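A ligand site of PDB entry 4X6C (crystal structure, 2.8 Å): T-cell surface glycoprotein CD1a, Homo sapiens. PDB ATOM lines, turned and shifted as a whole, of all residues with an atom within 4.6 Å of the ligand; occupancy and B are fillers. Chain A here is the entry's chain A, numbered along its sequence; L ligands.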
ATOM      1  N   PHE A   7       1.399 -16.190  18.046  1.00  0.00           N
ATOM      2  CA  PHE A   7       1.500 -15.076  17.121  1.00  0.00           C
ATOM      3  C   PHE A   7       1.878 -15.578  15.745  1.00  0.00           C
ATOM      4  O   PHE A   7       2.744 -16.426  15.628  1.00  0.00           O
ATOM      5  CB  PHE A   7       2.521 -14.035  17.581  1.00  0.00           C
ATOM      6  CG  PHE A   7       2.645 -12.881  16.638  1.00  0.00           C
ATOM      7  CD1 PHE A   7       1.748 -11.843  16.700  1.00  0.00           C
ATOM      8  CD2 PHE A   7       3.612 -12.855  15.656  1.00  0.00           C
ATOM      9  CE1 PHE A   7       1.832 -10.780  15.829  1.00  0.00           C
ATOM     10  CE2 PHE A   7       3.687 -11.810  14.777  1.00  0.00           C
ATOM     11  CZ  PHE A   7       2.799 -10.771  14.876  1.00  0.00           C
ATOM     12  N   VAL A   9       2.267 -14.516  11.243  1.00  0.00           N
ATOM     13  CA  VAL A   9       2.263 -13.635  10.108  1.00  0.00           C
ATOM     14  C   VAL A   9       1.695 -14.339   8.869  1.00  0.00           C
ATOM     15  O   VAL A   9       2.004 -15.497   8.651  1.00  0.00           O
ATOM     16  CB  VAL A   9       3.682 -13.195   9.807  1.00  0.00           C
ATOM     17  CG1 VAL A   9       3.735 -12.379   8.532  1.00  0.00           C
ATOM     18  CG2 VAL A   9       4.242 -12.416  10.978  1.00  0.00           C
ATOM     19  N   TRP A  11       1.295 -14.091   4.488  1.00  0.00           N
ATOM     20  CA  TRP A  11       1.545 -13.491   3.176  1.00  0.00           C
ATOM     21  C   TRP A  11       0.538 -14.036   2.174  1.00  0.00           C
ATOM     22  O   TRP A  11       0.259 -15.225   2.175  1.00  0.00           O
ATOM     23  CB  TRP A  11       2.942 -13.831   2.636  1.00  0.00           C
ATOM     24  CG  TRP A  11       4.145 -13.142   3.239  1.00  0.00           C
ATOM     25  CD1 TRP A  11       4.843 -12.098   2.691  1.00  0.00           C
ATOM     26  CD2 TRP A  11       4.858 -13.503   4.446  1.00  0.00           C
ATOM     27  NE1 TRP A  11       5.907 -11.768   3.494  1.00  0.00           N
ATOM     28  CE2 TRP A  11       5.938 -12.608   4.575  1.00  0.00           C
ATOM     29  CE3 TRP A  11       4.659 -14.470   5.446  1.00  0.00           C
ATOM     30  CZ2 TRP A  11       6.829 -12.664   5.655  1.00  0.00           C
ATOM     31  CZ3 TRP A  11       5.543 -14.515   6.507  1.00  0.00           C
ATOM     32  CH2 TRP A  11       6.605 -13.619   6.605  1.00  0.00           C
ATOM     33  N   VAL A  25       0.276  -8.397   3.629  1.00  0.00           N
ATOM     34  CA  VAL A  25       0.974  -9.042   4.746  1.00  0.00           C
ATOM     35  C   VAL A  25       0.464  -8.482   6.073  1.00  0.00           C
ATOM     36  O   VAL A  25       0.286  -7.275   6.211  1.00  0.00           O
ATOM     37  CB  VAL A  25       2.520  -8.851   4.696  1.00  0.00           C
ATOM     38  CG1 VAL A  25       3.183  -9.668   5.784  1.00  0.00           C
ATOM     39  CG2 VAL A  25       3.064  -9.281   3.373  1.00  0.00           C
ATOM     40  N   SER A  26       0.211  -9.357   7.041  1.00  0.00           N
ATOM     41  CA  SER A  26      -0.301  -8.919   8.333  1.00  0.00           C
ATOM     42  C   SER A  26       0.069  -9.842   9.490  1.00  0.00           C
ATOM     43  O   SER A  26       0.438 -11.019   9.301  1.00  0.00           O
ATOM     44  CB  SER A  26      -1.817  -8.778   8.273  1.00  0.00           C
ATOM     45  OG  SER A  26      -2.415 -10.007   7.894  1.00  0.00           O
ATOM     46  N   GLY A  27      -0.040  -9.293  10.699  1.00  0.00           N
ATOM     47  CA  GLY A  27       0.370  -9.979  11.905  1.00  0.00           C
ATOM     48  C   GLY A  27      -0.819 -10.143  12.824  1.00  0.00           C
ATOM     49  O   GLY A  27      -1.613  -9.221  13.034  1.00  0.00           O
ATOM     50  N   HIS A  35      -0.762  -6.203  13.398  1.00  0.00           N
ATOM     51  CA  HIS A  35       0.176  -5.504  12.511  1.00  0.00           C
ATOM     52  C   HIS A  35      -0.281  -5.524  11.071  1.00  0.00           C
ATOM     53  O   HIS A  35      -0.905  -6.473  10.607  1.00  0.00           O
ATOM     54  CB  HIS A  35       1.577  -6.110  12.613  1.00  0.00           C
ATOM     55  CG  HIS A  35       2.180  -6.008  13.965  1.00  0.00           C
ATOM     56  ND1 HIS A  35       1.856  -6.866  14.988  1.00  0.00           N
ATOM     57  CD2 HIS A  35       3.081  -5.135  14.472  1.00  0.00           C
ATOM     58  CE1 HIS A  35       2.543  -6.531  16.075  1.00  0.00           C
ATOM     59  NE2 HIS A  35       3.292  -5.485  15.784  1.00  0.00           N
ATOM     60  N   ILE A  44       6.202  -1.226   8.873  1.00  0.00           N
ATOM     61  CA  ILE A  44       5.208  -1.946   9.670  1.00  0.00           C
ATOM     62  C   ILE A  44       4.275  -0.996  10.412  1.00  0.00           C
ATOM     63  O   ILE A  44       4.724  -0.105  11.130  1.00  0.00           O
ATOM     64  CB  ILE A  44       5.885  -2.894  10.673  1.00  0.00           C
ATOM     65  CG1 ILE A  44       6.481  -4.094   9.942  1.00  0.00           C
ATOM     66  CG2 ILE A  44       4.888  -3.374  11.713  1.00  0.00           C
ATOM     67  CD1 ILE A  44       7.481  -4.877  10.760  1.00  0.00           C
ATOM     68  N   PHE A  55       9.962  -4.371  21.703  1.00  0.00           N
ATOM     69  CA  PHE A  55      10.977  -3.976  20.731  1.00  0.00           C
ATOM     70  C   PHE A  55      11.106  -2.457  20.654  1.00  0.00           C
ATOM     71  O   PHE A  55      10.140  -1.706  20.864  1.00  0.00           O
ATOM     72  CB  PHE A  55      10.679  -4.516  19.319  1.00  0.00           C
ATOM     73  CG  PHE A  55      11.020  -5.965  19.115  1.00  0.00           C
ATOM     74  CD1 PHE A  55      11.987  -6.587  19.889  1.00  0.00           C
ATOM     75  CD2 PHE A  55      10.382  -6.723  18.151  1.00  0.00           C
ATOM     76  CE1 PHE A  55      12.299  -7.934  19.716  1.00  0.00           C
ATOM     77  CE2 PHE A  55      10.693  -8.061  17.972  1.00  0.00           C
ATOM     78  CZ  PHE A  55      11.665  -8.649  18.759  1.00  0.00           C
ATOM     79  N   TRP A  60      12.637  -2.155  15.428  1.00  0.00           N
ATOM     80  CA  TRP A  60      11.563  -2.246  14.441  1.00  0.00           C
ATOM     81  C   TRP A  60      12.057  -1.779  13.079  1.00  0.00           C
ATOM     82  O   TRP A  60      11.671  -2.370  12.073  1.00  0.00           O
ATOM     83  CB  TRP A  60      10.340  -1.429  14.854  1.00  0.00           C
ATOM     84  CG  TRP A  60       9.444  -2.132  15.817  1.00  0.00           C
ATOM     85  CD1 TRP A  60       9.170  -1.762  17.102  1.00  0.00           C
ATOM     86  CD2 TRP A  60       8.700  -3.322  15.578  1.00  0.00           C
ATOM     87  NE1 TRP A  60       8.304  -2.642  17.676  1.00  0.00           N
ATOM     88  CE2 TRP A  60       7.997  -3.619  16.769  1.00  0.00           C
ATOM     89  CE3 TRP A  60       8.566  -4.179  14.488  1.00  0.00           C
ATOM     90  CZ2 TRP A  60       7.179  -4.734  16.885  1.00  0.00           C
ATOM     91  CZ3 TRP A  60       7.756  -5.276  14.612  1.00  0.00           C
ATOM     92  CH2 TRP A  60       7.075  -5.542  15.807  1.00  0.00           C
ATOM     93  N   LEU A  63      13.835  -4.719  11.722  1.00  0.00           N
ATOM     94  CA  LEU A  63      12.848  -5.715  11.303  1.00  0.00           C
ATOM     95  C   LEU A  63      12.087  -5.285  10.064  1.00  0.00           C
ATOM     96  O   LEU A  63      11.766  -6.114   9.213  1.00  0.00           O
ATOM     97  CB  LEU A  63      11.873  -6.031  12.435  1.00  0.00           C
ATOM     98  CG  LEU A  63      12.419  -6.947  13.527  1.00  0.00           C
ATOM     99  CD1 LEU A  63      11.495  -6.966  14.724  1.00  0.00           C
ATOM    100  CD2 LEU A  63      12.592  -8.341  12.960  1.00  0.00           C
ATOM    101  N   PHE A  67      12.347  -7.682   6.746  1.00  0.00           N
ATOM    102  CA  PHE A  67      11.229  -8.206   5.975  1.00  0.00           C
ATOM    103  C   PHE A  67      11.257  -7.738   4.536  1.00  0.00           C
ATOM    104  O   PHE A  67      11.107  -8.538   3.621  1.00  0.00           O
ATOM    105  CB  PHE A  67       9.899  -7.842   6.623  1.00  0.00           C
ATOM    106  CG  PHE A  67       9.489  -8.777   7.714  1.00  0.00           C
ATOM    107  CD1 PHE A  67      10.286  -9.881   8.021  1.00  0.00           C
ATOM    108  CD2 PHE A  67       8.305  -8.605   8.391  1.00  0.00           C
ATOM    109  CE1 PHE A  67       9.913 -10.759   9.008  1.00  0.00           C
ATOM    110  CE2 PHE A  67       7.925  -9.489   9.389  1.00  0.00           C
ATOM    111  CZ  PHE A  67       8.737 -10.568   9.693  1.00  0.00           C
ATOM    112  N   ARG A  70      13.841  -9.556   2.560  1.00  0.00           N
ATOM    113  CA  ARG A  70      13.564 -10.966   2.454  1.00  0.00           C
ATOM    114  C   ARG A  70      12.295 -11.245   1.662  1.00  0.00           C
ATOM    115  O   ARG A  70      12.242 -12.186   0.876  1.00  0.00           O
ATOM    116  CB  ARG A  70      13.501 -11.589   3.835  1.00  0.00           C
ATOM    117  CG  ARG A  70      14.091 -12.950   3.848  1.00  0.00           C
ATOM    118  CD  ARG A  70      14.729 -13.246   5.165  1.00  0.00           C
ATOM    119  NE  ARG A  70      14.944 -14.679   5.313  1.00  0.00           N
ATOM    120  CZ  ARG A  70      15.888 -15.358   4.660  1.00  0.00           C
ATOM    121  NH1 ARG A  70      16.681 -14.745   3.803  1.00  0.00           N
ATOM    122  NH2 ARG A  70      16.018 -16.653   4.867  1.00  0.00           N
ATOM    123  N   ARG A  73      13.454 -10.784  -2.155  1.00  0.00           N
ATOM    124  CA  ARG A  73      14.298 -11.876  -2.640  1.00  0.00           C
ATOM    125  C   ARG A  73      13.491 -13.162  -2.844  1.00  0.00           C
ATOM    126  O   ARG A  73      13.781 -13.982  -3.721  1.00  0.00           O
ATOM    127  CB  ARG A  73      15.460 -12.134  -1.680  1.00  0.00           C
ATOM    128  CG  ARG A  73      16.850 -11.858  -2.230  1.00  0.00           C
ATOM    129  CD  ARG A  73      17.872 -12.302  -1.209  1.00  0.00           C
ATOM    130  NE  ARG A  73      18.949 -11.333  -0.972  1.00  0.00           N
ATOM    131  CZ  ARG A  73      19.602 -11.208   0.189  1.00  0.00           C
ATOM    132  NH1 ARG A  73      19.293 -11.983   1.224  1.00  0.00           N
ATOM    133  NH2 ARG A  73      20.563 -10.300   0.310  1.00  0.00           N
ATOM    134  N   SER A  74      12.479 -13.341  -2.003  1.00  0.00           N
ATOM    135  CA  SER A  74      11.650 -14.534  -1.996  1.00  0.00           C
ATOM    136  C   SER A  74      10.681 -14.597  -3.160  1.00  0.00           C
ATOM    137  O   SER A  74      10.734 -15.538  -3.968  1.00  0.00           O
ATOM    138  CB  SER A  74      10.884 -14.608  -0.682  1.00  0.00           C
ATOM    139  OG  SER A  74      10.380 -13.322  -0.343  1.00  0.00           O
ATOM    140  N   GLY A  77      12.222 -15.067  -6.314  1.00  0.00           N
ATOM    141  CA  GLY A  77      12.692 -16.417  -6.561  1.00  0.00           C
ATOM    142  C   GLY A  77      11.648 -17.229  -7.306  1.00  0.00           C
ATOM    143  O   GLY A  77      11.955 -18.032  -8.180  1.00  0.00           O
ATOM    144  N   ARG A  80      11.649 -16.184 -10.723  1.00  0.00           N
ATOM    145  CA  ARG A  80      12.878 -16.733 -11.281  1.00  0.00           C
ATOM    146  C   ARG A  80      12.676 -18.171 -11.763  1.00  0.00           C
ATOM    147  O   ARG A  80      13.267 -18.589 -12.760  1.00  0.00           O
ATOM    148  CB  ARG A  80      13.994 -16.705 -10.216  1.00  0.00           C
ATOM    149  CG  ARG A  80      15.363 -17.217 -10.627  1.00  0.00           C
ATOM    150  CD  ARG A  80      16.242 -17.261  -9.368  1.00  0.00           C
ATOM    151  NE  ARG A  80      17.568 -17.827  -9.583  1.00  0.00           N
ATOM    152  CZ  ARG A  80      18.462 -18.016  -8.608  1.00  0.00           C
ATOM    153  NH1 ARG A  80      18.147 -17.707  -7.348  1.00  0.00           N
ATOM    154  NH2 ARG A  80      19.652 -18.539  -8.873  1.00  0.00           N
ATOM    155  N   TYR A  81      11.815 -18.900 -11.060  1.00  0.00           N
ATOM    156  CA  TYR A  81      11.556 -20.317 -11.339  1.00  0.00           C
ATOM    157  C   TYR A  81      10.104 -20.531 -11.715  1.00  0.00           C
ATOM    158  O   TYR A  81       9.561 -21.627 -11.556  1.00  0.00           O
ATOM    159  CB  TYR A  81      11.901 -21.200 -10.120  1.00  0.00           C
ATOM    160  CG  TYR A  81      13.387 -21.414  -9.874  1.00  0.00           C
ATOM    161  CD1 TYR A  81      14.059 -20.737  -8.856  1.00  0.00           C
ATOM    162  CD2 TYR A  81      14.120 -22.294 -10.667  1.00  0.00           C
ATOM    163  CE1 TYR A  81      15.412 -20.931  -8.644  1.00  0.00           C
ATOM    164  CE2 TYR A  81      15.491 -22.502 -10.459  1.00  0.00           C
ATOM    165  CZ  TYR A  81      16.131 -21.815  -9.439  1.00  0.00           C
ATOM    166  OH  TYR A  81      17.476 -22.008  -9.222  1.00  0.00           O
ATOM    167  N   GLY A  97       3.352 -18.098   9.065  1.00  0.00           N
ATOM    168  CA  GLY A  97       4.503 -18.437   9.874  1.00  0.00           C
ATOM    169  C   GLY A  97       4.408 -17.785  11.229  1.00  0.00           C
ATOM    170  O   GLY A  97       3.878 -16.697  11.358  1.00  0.00           O
ATOM    171  N   GLY A  98       4.931 -18.468  12.241  1.00  0.00           N
ATOM    172  CA  GLY A  98       4.834 -17.955  13.589  1.00  0.00           C
ATOM    173  C   GLY A  98       5.274 -18.936  14.665  1.00  0.00           C
ATOM    174  O   GLY A  98       5.923 -19.960  14.409  1.00  0.00           O
ATOM    175  N   LEU A 111       6.178 -22.650   9.674  1.00  0.00           N
ATOM    176  CA  LEU A 111       6.171 -21.794   8.503  1.00  0.00           C
ATOM    177  C   LEU A 111       5.672 -22.676   7.382  1.00  0.00           C
ATOM    178  O   LEU A 111       6.312 -23.685   7.061  1.00  0.00           O
ATOM    179  CB  LEU A 111       7.555 -21.220   8.209  1.00  0.00           C
ATOM    180  CG  LEU A 111       7.655 -20.401   6.911  1.00  0.00           C
ATOM    181  CD1 LEU A 111       6.751 -19.205   6.955  1.00  0.00           C
ATOM    182  CD2 LEU A 111       9.063 -19.956   6.673  1.00  0.00           C
ATOM    183  N   TRP A 128      13.439 -27.161   4.259  1.00  0.00           N
ATOM    184  CA  TRP A 128      12.110 -27.296   3.652  1.00  0.00           C
ATOM    185  C   TRP A 128      11.770 -28.715   3.228  1.00  0.00           C
ATOM    186  O   TRP A 128      12.509 -29.325   2.453  1.00  0.00           O
ATOM    187  CB  TRP A 128      12.007 -26.359   2.443  1.00  0.00           C
ATOM    188  CG  TRP A 128      12.038 -24.889   2.794  1.00  0.00           C
ATOM    189  CD1 TRP A 128      13.132 -24.082   2.863  1.00  0.00           C
ATOM    190  CD2 TRP A 128      10.906 -24.041   3.127  1.00  0.00           C
ATOM    191  NE1 TRP A 128      12.770 -22.808   3.208  1.00  0.00           N
ATOM    192  CE2 TRP A 128      11.407 -22.759   3.373  1.00  0.00           C
ATOM    193  CE3 TRP A 128       9.535 -24.257   3.227  1.00  0.00           C
ATOM    194  CZ2 TRP A 128      10.579 -21.690   3.731  1.00  0.00           C
ATOM    195  CZ3 TRP A 128       8.712 -23.205   3.579  1.00  0.00           C
ATOM    196  CH2 TRP A 128       9.244 -21.931   3.823  1.00  0.00           C
ATOM    197  N   VAL A 144      15.457 -26.250  -4.480  1.00  0.00           N
ATOM    198  CA  VAL A 144      15.715 -24.849  -4.755  1.00  0.00           C
ATOM    199  C   VAL A 144      15.870 -24.026  -3.489  1.00  0.00           C
ATOM    200  O   VAL A 144      16.807 -23.238  -3.359  1.00  0.00           O
ATOM    201  CB  VAL A 144      14.595 -24.229  -5.589  1.00  0.00           C
ATOM    202  CG1 VAL A 144      14.860 -22.759  -5.820  1.00  0.00           C
ATOM    203  CG2 VAL A 144      14.443 -24.975  -6.904  1.00  0.00           C
ATOM    204  N   LEU A 145      14.942 -24.215  -2.556  1.00  0.00           N
ATOM    205  CA  LEU A 145      14.913 -23.425  -1.332  1.00  0.00           C
ATOM    206  C   LEU A 145      16.034 -23.798  -0.353  1.00  0.00           C
ATOM    207  O   LEU A 145      16.465 -22.966   0.442  1.00  0.00           O
ATOM    208  CB  LEU A 145      13.553 -23.573  -0.639  1.00  0.00           C
ATOM    209  CG  LEU A 145      12.435 -22.774  -1.320  1.00  0.00           C
ATOM    210  CD1 LEU A 145      11.111 -23.077  -0.664  1.00  0.00           C
ATOM    211  CD2 LEU A 145      12.694 -21.282  -1.341  1.00  0.00           C
ATOM    212  N   GLU A 151      20.685 -18.989   4.325  1.00  0.00           N
ATOM    213  CA  GLU A 151      19.353 -18.403   4.231  1.00  0.00           C
ATOM    214  C   GLU A 151      18.401 -19.149   5.197  1.00  0.00           C
ATOM    215  O   GLU A 151      17.656 -18.535   5.960  1.00  0.00           O
ATOM    216  CB  GLU A 151      18.821 -18.446   2.792  1.00  0.00           C
ATOM    217  CG  GLU A 151      19.741 -17.766   1.756  1.00  0.00           C
ATOM    218  CD  GLU A 151      19.246 -16.390   1.284  1.00  0.00           C
ATOM    219  OE1 GLU A 151      18.608 -15.662   2.083  1.00  0.00           O
ATOM    220  OE2 GLU A 151      19.505 -16.054   0.102  1.00  0.00           O
ATOM    221  N   THR A 155      15.900 -17.901   8.581  1.00  0.00           N
ATOM    222  CA  THR A 155      14.516 -18.289   8.754  1.00  0.00           C
ATOM    223  C   THR A 155      14.313 -18.908  10.135  1.00  0.00           C
ATOM    224  O   THR A 155      13.433 -18.520  10.883  1.00  0.00           O
ATOM    225  CB  THR A 155      14.053 -19.281   7.680  1.00  0.00           C
ATOM    226  OG1 THR A 155      14.252 -18.719   6.377  1.00  0.00           O
ATOM    227  CG2 THR A 155      12.596 -19.658   7.885  1.00  0.00           C
ATOM    228  N   LEU A 158      14.461 -16.455  13.111  1.00  0.00           N
ATOM    229  CA  LEU A 158      13.259 -15.677  13.287  1.00  0.00           C
ATOM    230  C   LEU A 158      12.157 -16.514  13.902  1.00  0.00           C
ATOM    231  O   LEU A 158      11.490 -16.085  14.843  1.00  0.00           O
ATOM    232  CB  LEU A 158      12.808 -15.088  11.966  1.00  0.00           C
ATOM    233  CG  LEU A 158      13.828 -14.144  11.327  1.00  0.00           C
ATOM    234  CD1 LEU A 158      13.431 -13.822   9.926  1.00  0.00           C
ATOM    235  CD2 LEU A 158      13.985 -12.888  12.139  1.00  0.00           C
ATOM    236  N   LEU A 159      11.992 -17.742  13.416  1.00  0.00           N
ATOM    237  CA  LEU A 159      10.896 -18.597  13.863  1.00  0.00           C
ATOM    238  C   LEU A 159      11.072 -19.048  15.283  1.00  0.00           C
ATOM    239  O   LEU A 159      10.135 -18.994  16.073  1.00  0.00           O
ATOM    240  CB  LEU A 159      10.786 -19.824  12.976  1.00  0.00           C
ATOM    241  CG  LEU A 159       9.667 -19.912  11.932  1.00  0.00           C
ATOM    242  CD1 LEU A 159       8.944 -18.597  11.684  1.00  0.00           C
ATOM    243  CD2 LEU A 159      10.253 -20.445  10.645  1.00  0.00           C
ATOM    244  N   THR A 162      13.552 -15.130  17.530  1.00  0.00           N
ATOM    245  CA  THR A 162      12.936 -13.809  17.448  1.00  0.00           C
ATOM    246  C   THR A 162      11.489 -13.828  17.867  1.00  0.00           C
ATOM    247  O   THR A 162      11.063 -13.097  18.770  1.00  0.00           O
ATOM    248  CB  THR A 162      12.950 -13.227  16.018  1.00  0.00           C
ATOM    249  OG1 THR A 162      14.255 -13.354  15.452  1.00  0.00           O
ATOM    250  CG2 THR A 162      12.522 -11.730  16.026  1.00  0.00           C
ATOM    251  N   CYS A 163      10.735 -14.693  17.181  1.00  0.00           N
ATOM    252  CA  CYS A 163       9.300 -14.728  17.380  1.00  0.00           C
ATOM    253  C   CYS A 163       8.936 -14.983  18.860  1.00  0.00           C
ATOM    254  O   CYS A 163       8.171 -14.209  19.435  1.00  0.00           O
ATOM    255  CB  CYS A 163       8.676 -15.772  16.440  1.00  0.00           C
ATOM    256  SG  CYS A 163       6.870 -15.700  16.270  1.00  0.00           S
ATOM    257  N   PHE A 166       9.492 -11.961  21.086  1.00  0.00           N
ATOM    258  CA  PHE A 166       8.520 -10.958  20.741  1.00  0.00           C
ATOM    259  C   PHE A 166       7.169 -11.229  21.377  1.00  0.00           C
ATOM    260  O   PHE A 166       6.664 -10.398  22.140  1.00  0.00           O
ATOM    261  CB  PHE A 166       8.382 -10.887  19.223  1.00  0.00           C
ATOM    262  CG  PHE A 166       7.290  -9.979  18.748  1.00  0.00           C
ATOM    263  CD1 PHE A 166       7.255  -8.655  19.131  1.00  0.00           C
ATOM    264  CD2 PHE A 166       6.296 -10.459  17.907  1.00  0.00           C
ATOM    265  CE1 PHE A 166       6.245  -7.812  18.705  1.00  0.00           C
ATOM    266  CE2 PHE A 166       5.293  -9.609  17.470  1.00  0.00           C
ATOM    267  CZ  PHE A 166       5.271  -8.291  17.878  1.00  0.00           C
HETATM  268  O1  LIG L   1      10.680 -14.130   5.785  1.00  0.00           O
HETATM  269  C1  LIG L   1      11.010 -15.250   6.042  1.00  0.00           C
HETATM  270  O2  LIG L   1      12.066 -15.854   5.512  1.00  0.00           O
HETATM  271  C2  LIG L   1      11.835 -16.819   4.463  1.00  0.00           C
HETATM  272  C3  LIG L   1      13.141 -17.015   3.743  1.00  0.00           C
HETATM  273  C4  LIG L   1      13.161 -16.524   2.321  1.00  0.00           C
HETATM  274  O3  LIG L   1      14.250 -17.168   1.618  1.00  0.00           O
HETATM  275  P1  LIG L   1      14.640 -16.693   0.150  1.00  0.00           P
HETATM  276  O4  LIG L   1      15.500 -15.507   0.304  1.00  0.00           O
HETATM  277  O5  LIG L   1      15.521 -17.833  -0.519  1.00  0.00           O
HETATM  278  C5  LIG L   1      15.996 -17.657  -1.872  1.00  0.00           C
HETATM  279  C6  LIG L   1      15.284 -18.699  -2.700  1.00  0.00           C
HETATM  280  N1  LIG L   1      14.260 -18.176  -3.695  1.00  0.00           N
HETATM  281  C7  LIG L   1      12.995 -17.844  -2.981  1.00  0.00           C
HETATM  282  C8  LIG L   1      14.788 -16.940  -4.356  1.00  0.00           C
HETATM  283  C9  LIG L   1      13.968 -19.189  -4.748  1.00  0.00           C
HETATM  284  O6  LIG L   1      13.376 -16.583  -0.614  1.00  0.00           O
HETATM  285  O7  LIG L   1      13.483 -18.398   3.740  1.00  0.00           O
HETATM  286  C10 LIG L   1      10.297 -16.139   7.015  1.00  0.00           C
HETATM  287  C11 LIG L   1       9.427 -15.374   7.989  1.00  0.00           C
HETATM  288  C12 LIG L   1       9.290 -16.060   9.330  1.00  0.00           C
HETATM  289  C13 LIG L   1       9.179 -15.125  10.514  1.00  0.00           C
HETATM  290  C14 LIG L   1       7.750 -14.808  10.903  1.00  0.00           C
HETATM  291  C15 LIG L   1       7.578 -14.676  12.390  1.00  0.00           C
HETATM  292  C16 LIG L   1       7.643 -13.267  12.911  1.00  0.00           C
HETATM  293  C17 LIG L   1       8.947 -12.915  13.484  1.00  0.00           C
HETATM  294  C18 LIG L   1       9.210 -12.008  14.406  1.00  0.00           C
HETATM  295  C19 LIG L   1       8.252 -11.122  15.113  1.00  0.00           C
HETATM  296  C20 LIG L   1       8.179  -9.702  14.598  1.00  0.00           C
HETATM  297  C21 LIG L   1       7.381  -9.583  13.323  1.00  0.00           C
HETATM  298  C22 LIG L   1       6.046  -8.913  13.477  1.00  0.00           C
HETATM  299  C23 LIG L   1       5.730  -7.978  12.328  1.00  0.00           C
HETATM  300  C24 LIG L   1       4.473  -8.300  11.576  1.00  0.00           C
HETATM  301  C25 LIG L   1       4.584  -8.077  10.120  1.00  0.00           C
HETATM  302  C26 LIG L   1       3.360  -7.556   9.519  1.00  0.00           C
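Phe 7 touches the ligand. Trp 11 touches the ligand. N of Gly 27 touches C26 of the ligand, 3.996 Å away. CB of His 35 touches C24 of the ligand (3.8 Å). Ile 44 touches the ligand (CD1 to C23, 3.9 Å). Phe 67 touches the ligand (CE2 to C25, 3.7 Å). Arg 73 touches the ligand (O to C8, 3.2 Å). CA of Ser 74 touches O6 of the ligand, at 3.0 Å. Gly 77 touches the ligand. Val 144 touches the ligand. Leu 145 touches the ligand (CD2 to C7, 3.8 Å). Glu 151 touches the ligand. CB of Leu 158 touches C13 of the ligand (3.9 Å). Leu 159 touches the ligand. CG2 of Thr 162 touches C18 of the ligand, at 3.7 Å. Phe 166 touches the ligand (CD2 to C19, 3.5 Å). Hydrophobic or aromatic side chains within 4 Å of the ligand: Phe 7, Trp 11, His 35, Ile 44, Phe 67, Val 144, Leu 145, Leu 158, Leu 159 and Phe 166. Within 4 Å of the ligand: Phe 7, Trp 11, Gly 27, His 35, Ile 44, Phe 67, Arg 70, Arg 73, Ser 74, Gly 77, Val 144, Leu 145, Glu 151, Thr 155, Leu 158, Leu 159, Thr 162 and Phe 166. The nearest printed residue that does not touch the ligand is Val 9 (4.003 Å).
An oxygen (O4) of the ligand lies within salt-bridge range of the guanidinium group (NH1) of Arg 70, at 3.8 Å. The side-chain hydroxyl (OG1) of Thr 155 lies within hydrogen-bond range of an oxygen (O7) of the ligand (2.8 Å).
The side-chain hydroxyl (OG1) of Thr 155 is in hydrogen-bond range of the guanidinium group (NH2) of Arg 70. N of Gly 27 sits at hydrogen-bond distance from O of His 35 (3.0 Å). The guanidinium group of Arg 73 is in salt-bridge range of the side-chain carboxylate of Glu 151 (3.8 Å). The guanidinium group of Arg 70 is in salt-bridge range of the side-chain carboxylate of Glu 151 (2.7 Å). O of Leu 158 is in hydrogen-bond range of N of Cys 163, at 2.8 Å. OG of Ser 74 lies within hydrogen-bond range of O of Arg 70 (2.5 Å). The side-chain hydroxyl of Thr 155 is in hydrogen-bond range of the backbone carbonyl oxygen of Glu 151.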
